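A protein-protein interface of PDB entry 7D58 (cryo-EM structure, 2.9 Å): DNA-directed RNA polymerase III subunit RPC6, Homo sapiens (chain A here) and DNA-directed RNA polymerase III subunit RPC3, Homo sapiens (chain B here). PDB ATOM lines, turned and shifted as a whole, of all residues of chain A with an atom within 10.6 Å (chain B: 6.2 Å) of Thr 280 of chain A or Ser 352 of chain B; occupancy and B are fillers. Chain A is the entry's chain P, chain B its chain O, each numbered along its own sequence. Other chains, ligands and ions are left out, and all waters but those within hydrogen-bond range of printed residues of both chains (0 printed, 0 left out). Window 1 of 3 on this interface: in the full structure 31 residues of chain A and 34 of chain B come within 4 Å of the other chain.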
ATOM      1  N   TYR A 244       6.618  14.708  20.992  1.00  0.00           N
ATOM      2  CA  TYR A 244       6.681  14.885  19.545  1.00  0.00           C
ATOM      3  C   TYR A 244       7.831  14.091  18.941  1.00  0.00           C
ATOM      4  O   TYR A 244       7.725  13.617  17.804  1.00  0.00           O
ATOM      5  CB  TYR A 244       6.822  16.367  19.191  1.00  0.00           C
ATOM      6  CG  TYR A 244       5.710  17.243  19.725  1.00  0.00           C
ATOM      7  CD1 TYR A 244       4.421  16.748  19.874  1.00  0.00           C
ATOM      8  CD2 TYR A 244       5.951  18.562  20.085  1.00  0.00           C
ATOM      9  CE1 TYR A 244       3.402  17.544  20.365  1.00  0.00           C
ATOM     10  CE2 TYR A 244       4.940  19.364  20.582  1.00  0.00           C
ATOM     11  CZ  TYR A 244       3.668  18.851  20.716  1.00  0.00           C
ATOM     12  OH  TYR A 244       2.657  19.647  21.204  1.00  0.00           O
ATOM     13  N   ASP A 245       8.933  13.941  19.680  1.00  0.00           N
ATOM     14  CA  ASP A 245      10.040  13.119  19.204  1.00  0.00           C
ATOM     15  C   ASP A 245       9.654  11.646  19.167  1.00  0.00           C
ATOM     16  O   ASP A 245      10.142  10.887  18.322  1.00  0.00           O
ATOM     17  CB  ASP A 245      11.268  13.322  20.093  1.00  0.00           C
ATOM     18  CG  ASP A 245      11.986  14.626  19.808  1.00  0.00           C
ATOM     19  OD1 ASP A 245      12.857  15.013  20.615  1.00  0.00           O
ATOM     20  OD2 ASP A 245      11.683  15.262  18.779  1.00  0.00           O
ATOM     21  N   GLY A 246       8.783  11.222  20.081  1.00  0.00           N
ATOM     22  CA  GLY A 246       8.393   9.830  20.175  1.00  0.00           C
ATOM     23  C   GLY A 246       9.265   9.055  21.140  1.00  0.00           C
ATOM     24  O   GLY A 246       9.661   7.919  20.861  1.00  0.00           O
ATOM     25  N   PRO A 275      11.085   2.778  21.401  1.00  0.00           N
ATOM     26  CA  PRO A 275      10.591   2.741  20.017  1.00  0.00           C
ATOM     27  C   PRO A 275       9.900   1.417  19.717  1.00  0.00           C
ATOM     28  O   PRO A 275      10.235   0.380  20.292  1.00  0.00           O
ATOM     29  CB  PRO A 275      11.862   2.921  19.175  1.00  0.00           C
ATOM     30  CG  PRO A 275      12.997   2.612  20.104  1.00  0.00           C
ATOM     31  CD  PRO A 275      12.533   3.044  21.457  1.00  0.00           C
ATOM     32  N   ILE A 276       8.933   1.462  18.800  1.00  0.00           N
ATOM     33  CA  ILE A 276       8.108   0.289  18.531  1.00  0.00           C
ATOM     34  C   ILE A 276       8.881  -0.740  17.719  1.00  0.00           C
ATOM     35  O   ILE A 276       9.101  -1.870  18.169  1.00  0.00           O
ATOM     36  CB  ILE A 276       6.807   0.703  17.819  1.00  0.00           C
ATOM     37  CG1 ILE A 276       6.051   1.741  18.649  1.00  0.00           C
ATOM     38  CG2 ILE A 276       5.934  -0.515  17.555  1.00  0.00           C
ATOM     39  CD1 ILE A 276       4.911   2.403  17.906  1.00  0.00           C
ATOM     40  N   ILE A 277       9.304  -0.375  16.515  1.00  0.00           N
ATOM     41  CA  ILE A 277      10.043  -1.293  15.653  1.00  0.00           C
ATOM     42  C   ILE A 277      11.401  -0.684  15.326  1.00  0.00           C
ATOM     43  O   ILE A 277      11.532   0.548  15.280  1.00  0.00           O
ATOM     44  CB  ILE A 277       9.246  -1.622  14.380  1.00  0.00           C
ATOM     45  CG1 ILE A 277       8.919  -0.347  13.601  1.00  0.00           C
ATOM     46  CG2 ILE A 277       7.978  -2.391  14.726  1.00  0.00           C
ATOM     47  CD1 ILE A 277       8.320  -0.603  12.233  1.00  0.00           C
ATOM     48  N   PRO A 278      12.433  -1.494  15.107  1.00  0.00           N
ATOM     49  CA  PRO A 278      13.752  -0.950  14.768  1.00  0.00           C
ATOM     50  C   PRO A 278      13.722  -0.260  13.416  1.00  0.00           C
ATOM     51  O   PRO A 278      12.743  -0.398  12.667  1.00  0.00           O
ATOM     52  CB  PRO A 278      14.652  -2.197  14.744  1.00  0.00           C
ATOM     53  CG  PRO A 278      13.722  -3.330  14.482  1.00  0.00           C
ATOM     54  CD  PRO A 278      12.439  -2.966  15.172  1.00  0.00           C
ATOM     55  N   PRO A 279      14.761   0.504  13.077  1.00  0.00           N
ATOM     56  CA  PRO A 279      14.800   1.154  11.761  1.00  0.00           C
ATOM     57  C   PRO A 279      14.626   0.148  10.634  1.00  0.00           C
ATOM     58  O   PRO A 279      15.213  -0.937  10.645  1.00  0.00           O
ATOM     59  CB  PRO A 279      16.186   1.804  11.735  1.00  0.00           C
ATOM     60  CG  PRO A 279      16.483   2.079  13.166  1.00  0.00           C
ATOM     61  CD  PRO A 279      15.880   0.933  13.934  1.00  0.00           C
ATOM     62  N   THR A 280      13.801   0.514   9.659  1.00  0.00           N
ATOM     63  CA  THR A 280      13.447  -0.400   8.584  1.00  0.00           C
ATOM     64  C   THR A 280      14.637  -0.663   7.668  1.00  0.00           C
ATOM     65  O   THR A 280      15.567   0.143   7.564  1.00  0.00           O
ATOM     66  CB  THR A 280      12.283   0.162   7.769  1.00  0.00           C
ATOM     67  OG1 THR A 280      12.008  -0.708   6.664  1.00  0.00           O
ATOM     68  CG2 THR A 280      12.618   1.554   7.248  1.00  0.00           C
ATOM     69  N   GLY A 281      14.598  -1.818   6.996  1.00  0.00           N
ATOM     70  CA  GLY A 281      15.599  -2.139   5.996  1.00  0.00           C
ATOM     71  C   GLY A 281      15.409  -1.424   4.677  1.00  0.00           C
ATOM     72  O   GLY A 281      16.225  -1.596   3.767  1.00  0.00           O
ATOM     73  N   LEU A 282      14.335  -0.641   4.554  1.00  0.00           N
ATOM     74  CA  LEU A 282      14.132   0.183   3.368  1.00  0.00           C
ATOM     75  C   LEU A 282      15.264   1.182   3.178  1.00  0.00           C
ATOM     76  O   LEU A 282      15.836   1.273   2.085  1.00  0.00           O
ATOM     77  CB  LEU A 282      12.799   0.926   3.480  1.00  0.00           C
ATOM     78  CG  LEU A 282      12.182   1.671   2.292  1.00  0.00           C
ATOM     79  CD1 LEU A 282      10.704   1.867   2.562  1.00  0.00           C
ATOM     80  CD2 LEU A 282      12.839   3.020   2.022  1.00  0.00           C
ATOM     81  N   VAL A 283      15.593   1.940   4.224  1.00  0.00           N
ATOM     82  CA  VAL A 283      16.523   3.055   4.084  1.00  0.00           C
ATOM     83  C   VAL A 283      17.978   2.605   4.137  1.00  0.00           C
ATOM     84  O   VAL A 283      18.873   3.387   3.792  1.00  0.00           O
ATOM     85  CB  VAL A 283      16.233   4.101   5.174  1.00  0.00           C
ATOM     86  CG1 VAL A 283      16.811   3.652   6.509  1.00  0.00           C
ATOM     87  CG2 VAL A 283      16.740   5.477   4.771  1.00  0.00           C
ATOM     88  N   ARG A 284      18.242   1.361   4.549  1.00  0.00           N
ATOM     89  CA  ARG A 284      19.622   0.893   4.647  1.00  0.00           C
ATOM     90  C   ARG A 284      20.280   0.790   3.276  1.00  0.00           C
ATOM     91  O   ARG A 284      21.511   0.844   3.177  1.00  0.00           O
ATOM     92  CB  ARG A 284      19.669  -0.452   5.370  1.00  0.00           C
ATOM     93  CG  ARG A 284      19.232  -0.371   6.822  1.00  0.00           C
ATOM     94  CD  ARG A 284      18.988  -1.744   7.417  1.00  0.00           C
ATOM     95  NE  ARG A 284      18.584  -1.651   8.817  1.00  0.00           N
ATOM     96  CZ  ARG A 284      18.073  -2.659   9.516  1.00  0.00           C
ATOM     97  NH1 ARG A 284      17.905  -3.844   8.948  1.00  0.00           N
ATOM     98  NH2 ARG A 284      17.732  -2.481  10.784  1.00  0.00           N
ATOM     99  N   ALA A 285      19.487   0.632   2.220  1.00  0.00           N
ATOM    100  CA  ALA A 285      20.022   0.732   0.875  1.00  0.00           C
ATOM    101  C   ALA A 285      20.238   2.201   0.512  1.00  0.00           C
ATOM    102  O   ALA A 285      19.465   3.070   0.922  1.00  0.00           O
ATOM    103  CB  ALA A 285      19.079   0.078  -0.130  1.00  0.00           C
ATOM    104  N   PRO A 286      21.290   2.506  -0.257  1.00  0.00           N
ATOM    105  CA  PRO A 286      21.557   3.911  -0.602  1.00  0.00           C
ATOM    106  C   PRO A 286      20.524   4.532  -1.526  1.00  0.00           C
ATOM    107  O   PRO A 286      20.520   5.761  -1.676  1.00  0.00           O
ATOM    108  CB  PRO A 286      22.936   3.853  -1.277  1.00  0.00           C
ATOM    109  CG  PRO A 286      23.052   2.458  -1.779  1.00  0.00           C
ATOM    110  CD  PRO A 286      22.308   1.594  -0.803  1.00  0.00           C
ATOM    111  N   GLY A 288      17.437   4.819  -0.908  1.00  0.00           N
ATOM    112  CA  GLY A 288      16.494   5.584  -0.108  1.00  0.00           C
ATOM    113  C   GLY A 288      17.009   6.969   0.233  1.00  0.00           C
ATOM    114  O   GLY A 288      16.228   7.917   0.360  1.00  0.00           O
ATOM    115  N   LEU A 289      18.326   7.109   0.384  1.00  0.00           N
ATOM    116  CA  LEU A 289      18.941   8.399   0.664  1.00  0.00           C
ATOM    117  C   LEU A 289      19.190   9.223  -0.591  1.00  0.00           C
ATOM    118  O   LEU A 289      19.539  10.403  -0.479  1.00  0.00           O
ATOM    119  CB  LEU A 289      20.276   8.216   1.400  1.00  0.00           C
ATOM    120  CG  LEU A 289      20.298   7.991   2.915  1.00  0.00           C
ATOM    121  CD1 LEU A 289      19.637   9.148   3.658  1.00  0.00           C
ATOM    122  CD2 LEU A 289      19.680   6.659   3.294  1.00  0.00           C
ATOM    123  N   THR B 347       2.561   3.610  10.312  1.00  0.00           N
ATOM    124  CA  THR B 347       2.904   4.954  10.764  1.00  0.00           C
ATOM    125  C   THR B 347       4.336   4.998  11.286  1.00  0.00           C
ATOM    126  O   THR B 347       5.106   5.904  10.949  1.00  0.00           O
ATOM    127  CB  THR B 347       1.923   5.410  11.845  1.00  0.00           C
ATOM    128  OG1 THR B 347       0.584   5.340  11.341  1.00  0.00           O
ATOM    129  CG2 THR B 347       2.221   6.839  12.256  1.00  0.00           C
ATOM    130  N   ALA B 348       4.705   4.015  12.113  1.00  0.00           N
ATOM    131  CA  ALA B 348       6.061   3.945  12.647  1.00  0.00           C
ATOM    132  C   ALA B 348       7.078   3.779  11.528  1.00  0.00           C
ATOM    133  O   ALA B 348       8.170   4.358  11.573  1.00  0.00           O
ATOM    134  CB  ALA B 348       6.170   2.795  13.647  1.00  0.00           C
ATOM    135  N   THR B 349       6.731   2.991  10.508  1.00  0.00           N
ATOM    136  CA  THR B 349       7.596   2.858   9.340  1.00  0.00           C
ATOM    137  C   THR B 349       7.789   4.200   8.641  1.00  0.00           C
ATOM    138  O   THR B 349       8.908   4.548   8.241  1.00  0.00           O
ATOM    139  CB  THR B 349       7.009   1.824   8.377  1.00  0.00           C
ATOM    140  OG1 THR B 349       6.996   0.538   9.008  1.00  0.00           O
ATOM    141  CG2 THR B 349       7.830   1.749   7.102  1.00  0.00           C
ATOM    142  N   LEU B 350       6.708   4.970   8.490  1.00  0.00           N
ATOM    143  CA  LEU B 350       6.819   6.277   7.846  1.00  0.00           C
ATOM    144  C   LEU B 350       7.694   7.228   8.657  1.00  0.00           C
ATOM    145  O   LEU B 350       8.539   7.939   8.093  1.00  0.00           O
ATOM    146  CB  LEU B 350       5.431   6.883   7.633  1.00  0.00           C
ATOM    147  CG  LEU B 350       4.483   6.158   6.676  1.00  0.00           C
ATOM    148  CD1 LEU B 350       3.059   6.676   6.828  1.00  0.00           C
ATOM    149  CD2 LEU B 350       4.960   6.305   5.242  1.00  0.00           C
ATOM    150  N   GLU B 351       7.502   7.269   9.981  1.00  0.00           N
ATOM    151  CA  GLU B 351       8.339   8.158  10.784  1.00  0.00           C
ATOM    152  C   GLU B 351       9.792   7.702  10.787  1.00  0.00           C
ATOM    153  O   GLU B 351      10.706   8.532  10.818  1.00  0.00           O
ATOM    154  CB  GLU B 351       7.835   8.311  12.224  1.00  0.00           C
ATOM    155  CG  GLU B 351       6.676   9.286  12.391  1.00  0.00           C
ATOM    156  CD  GLU B 351       5.351   8.621  12.673  1.00  0.00           C
ATOM    157  OE1 GLU B 351       5.349   7.423  13.013  1.00  0.00           O
ATOM    158  OE2 GLU B 351       4.311   9.304  12.560  1.00  0.00           O
ATOM    159  N   SER B 352      10.034   6.393  10.734  1.00  0.00           N
ATOM    160  CA  SER B 352      11.412   5.925  10.650  1.00  0.00           C
ATOM    161  C   SER B 352      12.053   6.324   9.328  1.00  0.00           C
ATOM    162  O   SER B 352      13.221   6.732   9.303  1.00  0.00           O
ATOM    163  CB  SER B 352      11.472   4.410  10.832  1.00  0.00           C
ATOM    164  OG  SER B 352      12.815   3.959  10.834  1.00  0.00           O
ATOM    165  N   VAL B 353      11.304   6.229   8.227  1.00  0.00           N
ATOM    166  CA  VAL B 353      11.841   6.647   6.936  1.00  0.00           C
ATOM    167  C   VAL B 353      12.155   8.138   6.935  1.00  0.00           C
ATOM    168  O   VAL B 353      13.248   8.549   6.514  1.00  0.00           O
ATOM    169  CB  VAL B 353      10.868   6.272   5.803  1.00  0.00           C
ATOM    170  CG1 VAL B 353      11.234   7.002   4.511  1.00  0.00           C
ATOM    171  CG2 VAL B 353      10.872   4.766   5.586  1.00  0.00           C
ATOM    172  N   VAL B 354      11.227   8.974   7.417  1.00  0.00           N
ATOM    173  CA  VAL B 354      11.480  10.415   7.425  1.00  0.00           C
ATOM    174  C   VAL B 354      12.582  10.796   8.409  1.00  0.00           C
ATOM    175  O   VAL B 354      13.295  11.780   8.176  1.00  0.00           O
ATOM    176  CB  VAL B 354      10.202  11.222   7.729  1.00  0.00           C
ATOM    177  CG1 VAL B 354       9.662  10.896   9.102  1.00  0.00           C
ATOM    178  CG2 VAL B 354      10.456  12.722   7.600  1.00  0.00           C
ATOM    179  N   GLN B 355      12.764  10.037   9.492  1.00  0.00           N
ATOM    180  CA  GLN B 355      13.840  10.305  10.434  1.00  0.00           C
ATOM    181  C   GLN B 355      15.203   9.885   9.912  1.00  0.00           C
ATOM    182  O   GLN B 355      16.200  10.552  10.213  1.00  0.00           O
ATOM    183  CB  GLN B 355      13.567   9.596  11.764  1.00  0.00           C
ATOM    184  CG  GLN B 355      14.560   9.930  12.861  1.00  0.00           C
ATOM    185  CD  GLN B 355      14.187   9.306  14.189  1.00  0.00           C
ATOM    186  OE1 GLN B 355      13.702   9.989  15.090  1.00  0.00           O
ATOM    187  NE2 GLN B 355      14.411   8.004  14.318  1.00  0.00           N
ATOM    188  N   GLU B 356      15.275   8.805   9.136  1.00  0.00           N
ATOM    189  CA  GLU B 356      16.553   8.396   8.567  1.00  0.00           C
ATOM    190  C   GLU B 356      16.941   9.274   7.383  1.00  0.00           C
ATOM    191  O   GLU B 356      18.128   9.550   7.176  1.00  0.00           O
ATOM    192  CB  GLU B 356      16.497   6.924   8.150  1.00  0.00           C
ATOM    193  CG  GLU B 356      16.256   5.956   9.306  1.00  0.00           C
ATOM    194  CD  GLU B 356      17.397   5.927  10.308  1.00  0.00           C
ATOM    195  OE1 GLU B 356      18.562   6.113   9.898  1.00  0.00           O
ATOM    196  OE2 GLU B 356      17.125   5.719  11.509  1.00  0.00           O
ATOM    197  N   ARG B 357      15.957   9.732   6.605  1.00  0.00           N
ATOM    198  CA  ARG B 357      16.264  10.563   5.444  1.00  0.00           C
ATOM    199  C   ARG B 357      16.452  12.026   5.840  1.00  0.00           C
ATOM    200  O   ARG B 357      17.515  12.613   5.609  1.00  0.00           O
ATOM    201  CB  ARG B 357      15.164  10.422   4.389  1.00  0.00           C
ATOM    202  CG  ARG B 357      15.616  10.806   2.990  1.00  0.00           C
ATOM    203  CD  ARG B 357      14.605  10.407   1.925  1.00  0.00           C
ATOM    204  NE  ARG B 357      14.619  11.329   0.792  1.00  0.00           N
ATOM    205  CZ  ARG B 357      13.673  11.384  -0.141  1.00  0.00           C
ATOM    206  NH1 ARG B 357      12.634  10.562  -0.084  1.00  0.00           N
ATOM    207  NH2 ARG B 357      13.770  12.255  -1.136  1.00  0.00           N
ATOM    208  N   ARG B 367       5.492  14.149  13.324  1.00  0.00           N
ATOM    209  CA  ARG B 367       4.623  13.590  14.354  1.00  0.00           C
ATOM    210  C   ARG B 367       3.744  14.654  14.999  1.00  0.00           C
ATOM    211  O   ARG B 367       2.590  14.372  15.346  1.00  0.00           O
ATOM    212  CB  ARG B 367       5.464  12.873  15.410  1.00  0.00           C
ATOM    213  CG  ARG B 367       6.268  11.721  14.834  1.00  0.00           C
ATOM    214  CD  ARG B 367       7.222  11.092  15.835  1.00  0.00           C
ATOM    215  NE  ARG B 367       8.299  10.372  15.158  1.00  0.00           N
ATOM    216  CZ  ARG B 367       9.104   9.495  15.749  1.00  0.00           C
ATOM    217  NH1 ARG B 367       8.955   9.219  17.035  1.00  0.00           N
ATOM    218  NH2 ARG B 367      10.058   8.891  15.053  1.00  0.00           N
ATOM    219  N   GLN B 515      16.290  -7.027   3.247  1.00  0.00           N
ATOM    220  CA  GLN B 515      15.891  -5.973   4.173  1.00  0.00           C
ATOM    221  C   GLN B 515      14.954  -4.974   3.506  1.00  0.00           C
ATOM    222  O   GLN B 515      14.149  -4.331   4.187  1.00  0.00           O
ATOM    223  CB  GLN B 515      17.125  -5.260   4.728  1.00  0.00           C
ATOM    224  CG  GLN B 515      18.178  -6.183   5.331  1.00  0.00           C
ATOM    225  CD  GLN B 515      17.725  -6.848   6.619  1.00  0.00           C
ATOM    226  OE1 GLN B 515      18.135  -7.968   6.928  1.00  0.00           O
ATOM    227  NE2 GLN B 515      16.884  -6.158   7.379  1.00  0.00           N
ATOM    228  N   GLU B 518      11.367  -7.048   2.935  1.00  0.00           N
ATOM    229  CA  GLU B 518      10.545  -7.201   4.132  1.00  0.00           C
ATOM    230  C   GLU B 518       9.723  -5.942   4.391  1.00  0.00           C
ATOM    231  O   GLU B 518       8.596  -6.018   4.902  1.00  0.00           O
ATOM    232  CB  GLU B 518      11.416  -7.544   5.344  1.00  0.00           C
ATOM    233  CG  GLU B 518      12.466  -6.504   5.710  1.00  0.00           C
ATOM    234  CD  GLU B 518      11.959  -5.476   6.708  1.00  0.00           C
ATOM    235  OE1 GLU B 518      12.544  -4.374   6.778  1.00  0.00           O
ATOM    236  OE2 GLU B 518      10.981  -5.771   7.428  1.00  0.00           O
ATOM    237  N   THR B 519      10.260  -4.776   4.018  1.00  0.00           N
ATOM    238  CA  THR B 519       9.523  -3.532   4.198  1.00  0.00           C
ATOM    239  C   THR B 519       8.311  -3.454   3.281  1.00  0.00           C
ATOM    240  O   THR B 519       7.269  -2.924   3.682  1.00  0.00           O
ATOM    241  CB  THR B 519      10.441  -2.333   3.959  1.00  0.00           C
ATOM    242  OG1 THR B 519      11.649  -2.494   4.712  1.00  0.00           O
ATOM    243  CG2 THR B 519       9.751  -1.047   4.388  1.00  0.00           C
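OG1 of Thr 519 of chain B is in hydrogen-bond range of N of Leu 282 of chain A (3.3 Å). The side-chain hydroxyl of Thr 519 of chain B lies within hydrogen-bond range of the side-chain hydroxyl of Thr 280 of chain A, at 2.7 Å. The guanidinium group (NH1) of Arg 284 of chain A lies close to the side-chain amide nitrogen (NE2) of Gln 515 of chain B (3.0 Å). The backbone carbonyl oxygen of Gln 515 of chain B sits close to the backbone carbonyl oxygen of Gly 281 of chain A. The side-chain carboxylate (OE1) of Glu 518 of chain B sits at hydrogen-bond distance from the backbone NH (N) of Gly 281 of chain A (3.3 Å). NH1 of Arg 367 of chain B sits at hydrogen-bond distance from O of Asp 245 of chain A, 2.4 Å away.
The backbone carbonyl oxygen (O) of Gln 515 of chain B is in hydrogen-bond range of the side-chain hydroxyl (OG1) of Thr 519 of chain B, at 3.1 Å. The backbone carbonyl oxygen of Pro 279 of chain A is in hydrogen-bond range of the guanidinium group of Arg 284 of chain A (3.0 Å). N of Leu 282 of chain A lies close to OG1 of Thr 280 of chain A (3.1 Å). The side-chain hydroxyl of Thr 519 of chain B is in hydrogen-bond range of the side-chain carboxylate of Glu 518 of chain B (2.9 Å).
CD of Arg 367 of chain B touches O of Tyr 244 of chain A (3.2 Å). OG1 of Thr 349 of chain B touches CD1 of Ile 277 of chain A, 3.7 Å away. Pro 279 of chain A touches Ser 352 of chain B (CA to OG, 3.6 Å). Ser 352 of chain B touches Thr 280 of chain A (OG to N, 3.8 Å). OE1 of Glu 518 of chain B touches OG1 of Thr 280 of chain A (3.7 Å). N of Gly 281 of chain A touches OG1 of Thr 519 of chain B, 3.8 Å away. Leu 282 of chain A touches Gln 515 of chain B (N to O, 3.7 Å). Val 283 of chain A touches Glu 356 of chain B. Gly 288 of chain A touches Arg 357 of chain B (O to CD, 3.4 Å). CD1 of Leu 289 of chain A touches O of Glu 356 of chain B, 3.8 Å away.
Printed residues of chain B within 4 Å of Thr 280 of chain A: Ser 352, Glu 518 and Thr 519. Ser 352 of chain B touches two residues of chain A. No residue of chain A comes within 4 Å of Ala 348 of chain B. Thr 349 of chain B touches just one residue of chain A: Ile 277 (3.7 Å). No residue of chain A comes within 4 Å of Gln 355 of chain B. Glu 356 of chain B touches just these residues of chain A: Val 283 (3.7 Å) and Leu 289 (3.8 Å). Of the printed residues of chain A, Thr 519 of chain B touches Thr 280 (2.7 Å), Gly 281 (3.8 Å) and Leu 282 (3.3 Å). Printed residues of chain B within 4 Å of Gly 288 of chain A: Arg 357 (3.4 Å). Of the printed residues of chain B, Ile 277 of chain A touches Thr 349 (3.7 Å). Of the printed residues of chain A, Glu 518 of chain B touches Thr 280 (3.7 Å) and Gly 281 (3.3 Å). Printed residues of chain B within 4 Å of Leu 289 of chain A: Glu 356 (3.8 Å). Of the printed residues of chain B, Arg 284 of chain A touches Gln 515 (3.0 Å). The nearest printed residue of chain B that does not touch Thr 280 of chain A is Val 353 of chain B (4.02 Å).
Printed residues of chain B that touch a printed residue of chain A: Thr 349, Ser 352, Glu 356, Arg 357, Arg 367, Gln 515, Glu 518 and Thr 519. Of the 17 printed residues of chain A, 12 touch a printed residue of chain B. Printed residues of chain A that touch a printed residue of chain B: Tyr 244, Asp 245, Gly 246, Ile 277, Pro 279, Thr 280, Gly 281, Leu 282, Val 283, Arg 284, Gly 288 and Leu 289. Hydrophobic or aromatic side chains of chain A within 4 Å of the printed part of chain B: Ile 277, Leu 282, Val 283 and Leu 289. Along chain A the printed residues that touch a printed residue of chain B span positions 244 to 289. Among the printed residues, 17 pairs touch across the chains. Among the printed residues, no Asp or Glu carboxylate lies within 4 Å of a Lys or Arg side-chain nitrogen of the other chain.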
